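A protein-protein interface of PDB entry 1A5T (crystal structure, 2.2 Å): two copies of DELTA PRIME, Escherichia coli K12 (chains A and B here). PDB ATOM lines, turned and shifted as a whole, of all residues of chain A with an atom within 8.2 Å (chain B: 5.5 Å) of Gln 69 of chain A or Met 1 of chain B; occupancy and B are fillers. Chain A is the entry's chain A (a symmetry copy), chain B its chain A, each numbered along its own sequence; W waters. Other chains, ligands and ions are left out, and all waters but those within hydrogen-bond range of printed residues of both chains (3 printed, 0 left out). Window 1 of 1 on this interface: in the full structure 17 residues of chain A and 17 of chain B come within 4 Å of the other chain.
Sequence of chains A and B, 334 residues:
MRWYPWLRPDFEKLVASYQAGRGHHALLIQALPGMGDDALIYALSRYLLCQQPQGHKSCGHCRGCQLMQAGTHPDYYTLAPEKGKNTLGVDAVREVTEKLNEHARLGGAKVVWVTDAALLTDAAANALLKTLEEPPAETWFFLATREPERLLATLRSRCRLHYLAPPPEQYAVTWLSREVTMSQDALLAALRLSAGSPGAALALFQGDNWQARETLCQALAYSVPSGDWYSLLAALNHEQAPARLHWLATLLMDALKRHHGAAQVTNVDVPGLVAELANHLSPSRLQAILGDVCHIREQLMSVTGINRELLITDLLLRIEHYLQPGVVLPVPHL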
ATOM      1  N   TYR A  42     -18.971 -29.959  13.703  1.00  0.00           N
ATOM      2  CA  TYR A  42     -19.773 -28.787  13.957  1.00  0.00           C
ATOM      3  C   TYR A  42     -19.077 -27.541  13.411  1.00  0.00           C
ATOM      4  O   TYR A  42     -19.700 -26.727  12.727  1.00  0.00           O
ATOM      5  CB  TYR A  42     -20.093 -28.642  15.434  1.00  0.00           C
ATOM      6  CG  TYR A  42     -21.159 -27.585  15.691  1.00  0.00           C
ATOM      7  CD1 TYR A  42     -22.409 -27.636  15.049  1.00  0.00           C
ATOM      8  CD2 TYR A  42     -20.902 -26.514  16.537  1.00  0.00           C
ATOM      9  CE1 TYR A  42     -23.378 -26.638  15.245  1.00  0.00           C
ATOM     10  CE2 TYR A  42     -21.852 -25.515  16.745  1.00  0.00           C
ATOM     11  CZ  TYR A  42     -23.091 -25.580  16.091  1.00  0.00           C
ATOM     12  OH  TYR A  42     -24.005 -24.569  16.291  1.00  0.00           O
ATOM     13  N   ARG A  46     -20.734 -25.210  10.678  1.00  0.00           N
ATOM     14  CA  ARG A  46     -20.855 -23.790  10.887  1.00  0.00           C
ATOM     15  C   ARG A  46     -20.180 -23.002   9.779  1.00  0.00           C
ATOM     16  O   ARG A  46     -20.722 -22.011   9.321  1.00  0.00           O
ATOM     17  CB  ARG A  46     -20.300 -23.405  12.254  1.00  0.00           C
ATOM     18  CG  ARG A  46     -21.188 -23.850  13.385  1.00  0.00           C
ATOM     19  CD  ARG A  46     -22.603 -23.272  13.218  1.00  0.00           C
ATOM     20  NE  ARG A  46     -22.588 -21.812  13.227  1.00  0.00           N
ATOM     21  CZ  ARG A  46     -22.616 -21.074  14.336  1.00  0.00           C
ATOM     22  NH1 ARG A  46     -22.692 -21.670  15.522  1.00  0.00           N
ATOM     23  NH2 ARG A  46     -22.457 -19.750  14.274  1.00  0.00           N
ATOM     24  N   SER A  58     -16.840 -18.945  11.019  1.00  0.00           N
ATOM     25  CA  SER A  58     -18.219 -18.567  10.858  1.00  0.00           C
ATOM     26  C   SER A  58     -18.206 -17.120  11.410  1.00  0.00           C
ATOM     27  O   SER A  58     -17.451 -16.839  12.339  1.00  0.00           O
ATOM     28  CB  SER A  58     -19.037 -19.460  11.780  1.00  0.00           C
ATOM     29  OG  SER A  58     -20.263 -19.794  11.180  1.00  0.00           O
ATOM     30  N   CYS A  59     -19.001 -16.195  10.872  1.00  0.00           N
ATOM     31  CA  CYS A  59     -18.952 -14.823  11.412  1.00  0.00           C
ATOM     32  C   CYS A  59     -19.641 -14.653  12.775  1.00  0.00           C
ATOM     33  O   CYS A  59     -19.210 -13.849  13.607  1.00  0.00           O
ATOM     34  CB  CYS A  59     -19.508 -13.820  10.400  1.00  0.00           C
ATOM     35  SG  CYS A  59     -21.247 -14.103   9.949  1.00  0.00           S
ATOM     36  N   GLY A  60     -20.723 -15.399  12.998  1.00  0.00           N
ATOM     37  CA  GLY A  60     -21.469 -15.311  14.256  1.00  0.00           C
ATOM     38  C   GLY A  60     -22.485 -14.178  14.304  1.00  0.00           C
ATOM     39  O   GLY A  60     -23.062 -13.920  15.351  1.00  0.00           O
ATOM     40  N   HIS A  61     -22.729 -13.555  13.150  1.00  0.00           N
ATOM     41  CA  HIS A  61     -23.638 -12.424  12.992  1.00  0.00           C
ATOM     42  C   HIS A  61     -24.688 -12.619  11.898  1.00  0.00           C
ATOM     43  O   HIS A  61     -25.852 -12.307  12.126  1.00  0.00           O
ATOM     44  CB  HIS A  61     -22.835 -11.165  12.678  1.00  0.00           C
ATOM     45  CG  HIS A  61     -21.877 -10.791  13.761  1.00  0.00           C
ATOM     46  ND1 HIS A  61     -20.508 -10.872  13.617  1.00  0.00           N
ATOM     47  CD2 HIS A  61     -22.099 -10.344  15.020  1.00  0.00           C
ATOM     48  CE1 HIS A  61     -19.929 -10.490  14.743  1.00  0.00           C
ATOM     49  NE2 HIS A  61     -20.870 -10.170  15.610  1.00  0.00           N
ATOM     50  N   CYS A  62     -24.295 -13.124  10.728  1.00  0.00           N
ATOM     51  CA  CYS A  62     -25.232 -13.332   9.616  1.00  0.00           C
ATOM     52  C   CYS A  62     -26.440 -14.124  10.091  1.00  0.00           C
ATOM     53  O   CYS A  62     -26.373 -14.787  11.134  1.00  0.00           O
ATOM     54  CB  CYS A  62     -24.561 -14.061   8.438  1.00  0.00           C
ATOM     55  SG  CYS A  62     -24.272 -15.872   8.660  1.00  0.00           S
ATOM     56  N   ARG A  63     -27.532 -14.085   9.332  1.00  0.00           N
ATOM     57  CA  ARG A  63     -28.753 -14.799   9.736  1.00  0.00           C
ATOM     58  C   ARG A  63     -28.583 -16.317   9.881  1.00  0.00           C
ATOM     59  O   ARG A  63     -29.185 -16.947  10.768  1.00  0.00           O
ATOM     60  CB  ARG A  63     -29.942 -14.464   8.812  1.00  0.00           C
ATOM     61  CG  ARG A  63     -31.268 -15.003   9.343  1.00  0.00           C
ATOM     62  CD  ARG A  63     -32.497 -14.399   8.672  1.00  0.00           C
ATOM     63  NE  ARG A  63     -33.202 -15.338   7.799  1.00  0.00           N
ATOM     64  CZ  ARG A  63     -34.104 -16.230   8.215  1.00  0.00           C
ATOM     65  NH1 ARG A  63     -34.427 -16.311   9.504  1.00  0.00           N
ATOM     66  NH2 ARG A  63     -34.676 -17.041   7.333  1.00  0.00           N
ATOM     67  N   GLY A  64     -27.741 -16.894   9.025  1.00  0.00           N
ATOM     68  CA  GLY A  64     -27.485 -18.328   9.061  1.00  0.00           C
ATOM     69  C   GLY A  64     -26.885 -18.725  10.384  1.00  0.00           C
ATOM     70  O   GLY A  64     -27.295 -19.716  10.983  1.00  0.00           O
ATOM     71  N   CYS A  65     -25.895 -17.956  10.831  1.00  0.00           N
ATOM     72  CA  CYS A  65     -25.248 -18.209  12.119  1.00  0.00           C
ATOM     73  C   CYS A  65     -26.250 -17.973  13.239  1.00  0.00           C
ATOM     74  O   CYS A  65     -26.226 -18.686  14.239  1.00  0.00           O
ATOM     75  CB  CYS A  65     -24.028 -17.293  12.313  1.00  0.00           C
ATOM     76  SG  CYS A  65     -22.594 -17.675  11.255  1.00  0.00           S
ATOM     77  N   GLN A  66     -27.113 -16.967  13.081  1.00  0.00           N
ATOM     78  CA  GLN A  66     -28.126 -16.659  14.093  1.00  0.00           C
ATOM     79  C   GLN A  66     -29.063 -17.859  14.275  1.00  0.00           C
ATOM     80  O   GLN A  66     -29.317 -18.294  15.394  1.00  0.00           O
ATOM     81  CB  GLN A  66     -28.906 -15.397  13.721  1.00  0.00           C
ATOM     82  CG  GLN A  66     -28.223 -14.030  14.042  1.00  0.00           C
ATOM     83  CD  GLN A  66     -29.119 -12.843  13.692  1.00  0.00           C
ATOM     84  OE1 GLN A  66     -30.237 -12.720  14.202  1.00  0.00           O
ATOM     85  NE2 GLN A  66     -28.653 -11.995  12.789  1.00  0.00           N
ATOM     86  N   LEU A  67     -29.584 -18.400  13.184  1.00  0.00           N
ATOM     87  CA  LEU A  67     -30.443 -19.574  13.270  1.00  0.00           C
ATOM     88  C   LEU A  67     -29.650 -20.798  13.795  1.00  0.00           C
ATOM     89  O   LEU A  67     -30.219 -21.664  14.452  1.00  0.00           O
ATOM     90  CB  LEU A  67     -31.057 -19.893  11.905  1.00  0.00           C
ATOM     91  CG  LEU A  67     -31.889 -18.806  11.246  1.00  0.00           C
ATOM     92  CD1 LEU A  67     -32.385 -19.358   9.934  1.00  0.00           C
ATOM     93  CD2 LEU A  67     -33.058 -18.411  12.126  1.00  0.00           C
ATOM     94  N   MET A  68     -28.353 -20.893  13.499  1.00  0.00           N
ATOM     95  CA  MET A  68     -27.596 -22.029  14.024  1.00  0.00           C
ATOM     96  C   MET A  68     -27.451 -21.867  15.531  1.00  0.00           C
ATOM     97  O   MET A  68     -27.670 -22.827  16.273  1.00  0.00           O
ATOM     98  CB  MET A  68     -26.217 -22.178  13.375  1.00  0.00           C
ATOM     99  CG  MET A  68     -26.186 -22.833  11.968  1.00  0.00           C
ATOM    100  SD  MET A  68     -26.812 -24.520  11.855  1.00  0.00           S
ATOM    101  CE  MET A  68     -25.359 -25.498  12.446  1.00  0.00           C
ATOM    102  N   GLN A  69     -27.103 -20.658  15.978  1.00  0.00           N
ATOM    103  CA  GLN A  69     -26.932 -20.361  17.415  1.00  0.00           C
ATOM    104  C   GLN A  69     -28.224 -20.700  18.137  1.00  0.00           C
ATOM    105  O   GLN A  69     -28.204 -21.188  19.261  1.00  0.00           O
ATOM    106  CB  GLN A  69     -26.657 -18.867  17.659  1.00  0.00           C
ATOM    107  CG  GLN A  69     -25.307 -18.327  17.159  1.00  0.00           C
ATOM    108  CD  GLN A  69     -25.326 -16.821  16.992  1.00  0.00           C
ATOM    109  OE1 GLN A  69     -26.380 -16.196  17.101  1.00  0.00           O
ATOM    110  NE2 GLN A  69     -24.171 -16.234  16.682  1.00  0.00           N
ATOM    111  N   ALA A  70     -29.351 -20.387  17.496  1.00  0.00           N
ATOM    112  CA  ALA A  70     -30.681 -20.657  18.045  1.00  0.00           C
ATOM    113  C   ALA A  70     -31.021 -22.142  17.983  1.00  0.00           C
ATOM    114  O   ALA A  70     -31.835 -22.633  18.769  1.00  0.00           O
ATOM    115  CB  ALA A  70     -31.713 -19.879  17.267  1.00  0.00           C
ATOM    116  N   GLY A  71     -30.445 -22.818  16.983  1.00  0.00           N
ATOM    117  CA  GLY A  71     -30.659 -24.238  16.765  1.00  0.00           C
ATOM    118  C   GLY A  71     -31.883 -24.430  15.896  1.00  0.00           C
ATOM    119  O   GLY A  71     -32.536 -25.472  15.948  1.00  0.00           O
ATOM    120  N   THR A  72     -32.143 -23.448  15.048  1.00  0.00           N
ATOM    121  CA  THR A  72     -33.304 -23.444  14.178  1.00  0.00           C
ATOM    122  C   THR A  72     -33.002 -23.365  12.685  1.00  0.00           C
ATOM    123  O   THR A  72     -33.919 -23.131  11.898  1.00  0.00           O
ATOM    124  CB  THR A  72     -34.222 -22.250  14.551  1.00  0.00           C
ATOM    125  OG1 THR A  72     -33.536 -21.006  14.310  1.00  0.00           O
ATOM    126  CG2 THR A  72     -34.601 -22.316  16.025  1.00  0.00           C
ATOM    127  N   HIS A  73     -31.746 -23.519  12.272  1.00  0.00           N
ATOM    128  CA  HIS A  73     -31.437 -23.455  10.830  1.00  0.00           C
ATOM    129  C   HIS A  73     -32.133 -24.587  10.041  1.00  0.00           C
ATOM    130  O   HIS A  73     -31.851 -25.764  10.261  1.00  0.00           O
ATOM    131  CB  HIS A  73     -29.925 -23.503  10.599  1.00  0.00           C
ATOM    132  CG  HIS A  73     -29.497 -22.877   9.312  1.00  0.00           C
ATOM    133  ND1 HIS A  73     -29.955 -23.299   8.083  1.00  0.00           N
ATOM    134  CD2 HIS A  73     -28.701 -21.815   9.062  1.00  0.00           C
ATOM    135  CE1 HIS A  73     -29.467 -22.524   7.137  1.00  0.00           C
ATOM    136  NE2 HIS A  73     -28.707 -21.612   7.707  1.00  0.00           N
ATOM    137  N   MET B   1     -31.192 -19.249  22.298  1.00  0.00           N
ATOM    138  CA  MET B   1     -30.354 -18.025  22.405  1.00  0.00           C
ATOM    139  C   MET B   1     -29.948 -17.653  21.001  1.00  0.00           C
ATOM    140  O   MET B   1     -29.675 -18.527  20.174  1.00  0.00           O
ATOM    141  CB  MET B   1     -29.131 -18.261  23.285  1.00  0.00           C
ATOM    142  CG  MET B   1     -28.435 -16.966  23.692  1.00  0.00           C
ATOM    143  SD  MET B   1     -26.995 -17.154  24.758  1.00  0.00           S
ATOM    144  CE  MET B   1     -27.708 -17.260  26.319  1.00  0.00           C
ATOM    145  N   ARG B   2     -29.940 -16.355  20.702  1.00  0.00           N
ATOM    146  CA  ARG B   2     -29.633 -15.908  19.355  1.00  0.00           C
ATOM    147  C   ARG B   2     -28.999 -14.540  19.389  1.00  0.00           C
ATOM    148  O   ARG B   2     -29.400 -13.681  20.179  1.00  0.00           O
ATOM    149  CB  ARG B   2     -30.939 -15.887  18.545  1.00  0.00           C
ATOM    150  CG  ARG B   2     -30.801 -15.339  17.154  1.00  0.00           C
ATOM    151  CD  ARG B   2     -32.072 -15.444  16.354  1.00  0.00           C
ATOM    152  NE  ARG B   2     -31.884 -14.782  15.067  1.00  0.00           N
ATOM    153  CZ  ARG B   2     -32.744 -14.837  14.056  1.00  0.00           C
ATOM    154  NH1 ARG B   2     -33.863 -15.528  14.193  1.00  0.00           N
ATOM    155  NH2 ARG B   2     -32.478 -14.208  12.911  1.00  0.00           N
ATOM    156  N   TRP B   3     -27.991 -14.325  18.549  1.00  0.00           N
ATOM    157  CA  TRP B   3     -27.346 -13.016  18.542  1.00  0.00           C
ATOM    158  C   TRP B   3     -28.048 -12.120  17.545  1.00  0.00           C
ATOM    159  O   TRP B   3     -27.735 -12.125  16.352  1.00  0.00           O
ATOM    160  CB  TRP B   3     -25.854 -13.099  18.216  1.00  0.00           C
ATOM    161  CG  TRP B   3     -25.141 -11.812  18.413  1.00  0.00           C
ATOM    162  CD1 TRP B   3     -24.656 -10.972  17.450  1.00  0.00           C
ATOM    163  CD2 TRP B   3     -24.819 -11.192  19.679  1.00  0.00           C
ATOM    164  NE1 TRP B   3     -24.053  -9.873  18.030  1.00  0.00           N
ATOM    165  CE2 TRP B   3     -24.140  -9.985  19.393  1.00  0.00           C
ATOM    166  CE3 TRP B   3     -25.048 -11.534  21.019  1.00  0.00           C
ATOM    167  CZ2 TRP B   3     -23.676  -9.123  20.396  1.00  0.00           C
ATOM    168  CZ3 TRP B   3     -24.588 -10.675  22.025  1.00  0.00           C
ATOM    169  CH2 TRP B   3     -23.913  -9.484  21.707  1.00  0.00           C
ATOM    170  N   ASP B  38     -30.299 -12.251  27.120  1.00  0.00           N
ATOM    171  CA  ASP B  38     -29.632 -13.485  27.396  1.00  0.00           C
ATOM    172  C   ASP B  38     -28.359 -13.632  26.546  1.00  0.00           C
ATOM    173  O   ASP B  38     -27.287 -13.946  27.078  1.00  0.00           O
ATOM    174  CB  ASP B  38     -30.621 -14.655  27.220  1.00  0.00           C
ATOM    175  CG  ASP B  38     -31.135 -14.832  25.774  1.00  0.00           C
ATOM    176  OD1 ASP B  38     -31.108 -13.872  24.971  1.00  0.00           O
ATOM    177  OD2 ASP B  38     -31.570 -15.963  25.421  1.00  0.00           O
ATOM    178  N   ALA B  39     -28.455 -13.319  25.255  1.00  0.00           N
ATOM    179  CA  ALA B  39     -27.322 -13.396  24.343  1.00  0.00           C
ATOM    180  C   ALA B  39     -26.284 -12.324  24.668  1.00  0.00           C
ATOM    181  O   ALA B  39     -25.074 -12.546  24.522  1.00  0.00           O
ATOM    182  CB  ALA B  39     -27.790 -13.242  22.905  1.00  0.00           C
ATOM    183  N   TYR B  42     -24.507 -13.301  27.827  1.00  0.00           N
ATOM    184  CA  TYR B  42     -23.642 -14.417  27.533  1.00  0.00           C
ATOM    185  C   TYR B  42     -22.386 -13.936  26.807  1.00  0.00           C
ATOM    186  O   TYR B  42     -21.271 -14.316  27.171  1.00  0.00           O
ATOM    187  CB  TYR B  42     -24.368 -15.487  26.737  1.00  0.00           C
ATOM    188  CG  TYR B  42     -23.572 -16.784  26.655  1.00  0.00           C
ATOM    189  CD1 TYR B  42     -23.117 -17.435  27.815  1.00  0.00           C
ATOM    190  CD2 TYR B  42     -23.237 -17.330  25.424  1.00  0.00           C
ATOM    191  CE1 TYR B  42     -22.342 -18.605  27.745  1.00  0.00           C
ATOM    192  CE2 TYR B  42     -22.470 -18.491  25.335  1.00  0.00           C
ATOM    193  CZ  TYR B  42     -22.021 -19.124  26.503  1.00  0.00           C
ATOM    194  OH  TYR B  42     -21.242 -20.256  26.391  1.00  0.00           O
ATOM    195  N   TRP B 113     -24.792 -15.060  36.656  1.00  0.00           N
ATOM    196  CA  TRP B 113     -25.918 -14.611  35.844  1.00  0.00           C
ATOM    197  C   TRP B 113     -27.220 -14.957  36.525  1.00  0.00           C
ATOM    198  O   TRP B 113     -27.540 -16.125  36.673  1.00  0.00           O
ATOM    199  CB  TRP B 113     -25.900 -15.283  34.467  1.00  0.00           C
ATOM    200  CG  TRP B 113     -27.031 -14.914  33.550  1.00  0.00           C
ATOM    201  CD1 TRP B 113     -27.974 -13.951  33.762  1.00  0.00           C
ATOM    202  CD2 TRP B 113     -27.340 -15.497  32.284  1.00  0.00           C
ATOM    203  NE1 TRP B 113     -28.848 -13.905  32.705  1.00  0.00           N
ATOM    204  CE2 TRP B 113     -28.486 -14.839  31.780  1.00  0.00           C
ATOM    205  CE3 TRP B 113     -26.756 -16.515  31.508  1.00  0.00           C
ATOM    206  CZ2 TRP B 113     -29.061 -15.159  30.556  1.00  0.00           C
ATOM    207  CZ3 TRP B 113     -27.334 -16.835  30.273  1.00  0.00           C
ATOM    208  CH2 TRP B 113     -28.473 -16.157  29.815  1.00  0.00           C
HETATM  209  O   HOH W   1     -26.374 -10.185  14.282  1.00  0.00           O
HETATM  210  O   HOH W   2     -29.054 -21.050  21.820  1.00  0.00           O
HETATM  211  O   HOH W   3     -22.014  -7.588  16.992  1.00  0.00           O
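The backbone carbonyl oxygen (O) of Met 1 of chain B sits close to the backbone NH (N) of Ala 70 of chain A (3.3 Å). NE of Arg 2 of chain B sits at hydrogen-bond distance from OE1 of Gln 66 of chain A. The side-chain amide oxygen (OE1) of Gln 66 of chain A sits close to the backbone carbonyl oxygen (O) of Trp 3 of chain B (3.4 Å). OE1 of Gln 69 of chain A is in hydrogen-bond range of N of Trp 3 of chain B (2.9 Å). O of Met 1 of chain B sits close to O of Gln 69 of chain A (3.2 Å).
A ring nitrogen (ND1) of His 61 of chain A lies within hydrogen-bond range of the backbone carbonyl oxygen of Cys 59 of chain A (3.2 Å). The backbone NH of Gly 60 of chain A lies close to the side-chain sulfur of Cys 65 of chain A, 3.4 Å away. The side-chain amide nitrogen of Gln 69 of chain A is in hydrogen-bond range of the backbone carbonyl oxygen of Gly 60 of chain A (2.9 Å). The side-chain amide nitrogen of Gln 66 of chain A sits at hydrogen-bond distance from the backbone carbonyl oxygen of His 61 of chain A (2.9 Å). O of Leu 67 of chain A sits at hydrogen-bond distance from N of Thr 72 of chain A (2.7 Å). The backbone carbonyl oxygen (O) of Leu 67 of chain A is in hydrogen-bond range of the backbone NH (N) of His 73 of chain A (3.2 Å).
Among the printed residues, pairs that only touch across the chains: Gly 60 of chain A with Trp 3 of chain B (3.95 Å), His 61 of chain A with Trp 3 of chain B (3.6 Å), Arg 63 of chain A with Arg 2 of chain B (3.9 Å), Leu 67 of chain A with Arg 2 of chain B (3.6 Å) and Gln 69 of chain A with Arg 2 of chain B (3.9 Å).
Gln 69 of chain A touches three residues of chain B. Of chain A, only Gln 69 and Ala 70 come within 4 Å of Met 1 of chain B. Printed residues of chain B within 4 Å of Gly 60 of chain A: Trp 3. Of the printed residues of chain B, His 61 of chain A touches Trp 3 (3.6 Å). Of the printed residues of chain A, Trp 3 of chain B touches Gly 60, His 61, Gln 66 and Gln 69. Of the printed residues of chain B, Ala 70 of chain A touches Met 1 (3.2 Å). Of the printed residues of chain B, Gln 66 of chain A touches Arg 2 and Trp 3.
Printed residues of chain A that touch a printed residue of chain B: Gly 60, His 61, Arg 63, Gln 66, Leu 67, Gln 69 and Ala 70. Of the 7 printed residues of chain B, 3 touch a printed residue of chain A. Printed residues of chain B that touch a printed residue of chain A: Met 1, Arg 2 and Trp 3. Hydrophobic or aromatic side chains of chain B within 4 Å of the printed part of chain A: Trp 3. Among the printed residues, 10 pairs touch across the chains. Among the printed residues, no Asp or Glu carboxylate lies within 4 Å of a Lys or Arg side-chain nitrogen of the other chain.
1 position is printed for both chains.
Water W2 lies within hydrogen-bond range of the backbone carbonyl oxygen of Gln 69 of chain A (2.7 Å) and the backbone NH of Met 1 of chain B (2.8 Å). Water W1 lies within hydrogen-bond range of the backbone carbonyl oxygen (O) of His 61 of chain A, the backbone carbonyl oxygen (O) of Trp 3 of chain B and the side-chain amide nitrogen (NE2) of Gln 66 of chain A. Water W3 bridges NE2 of His 61 of chain A (3.1 Å) and NE1 of Trp 3 of chain B (3.2 Å).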
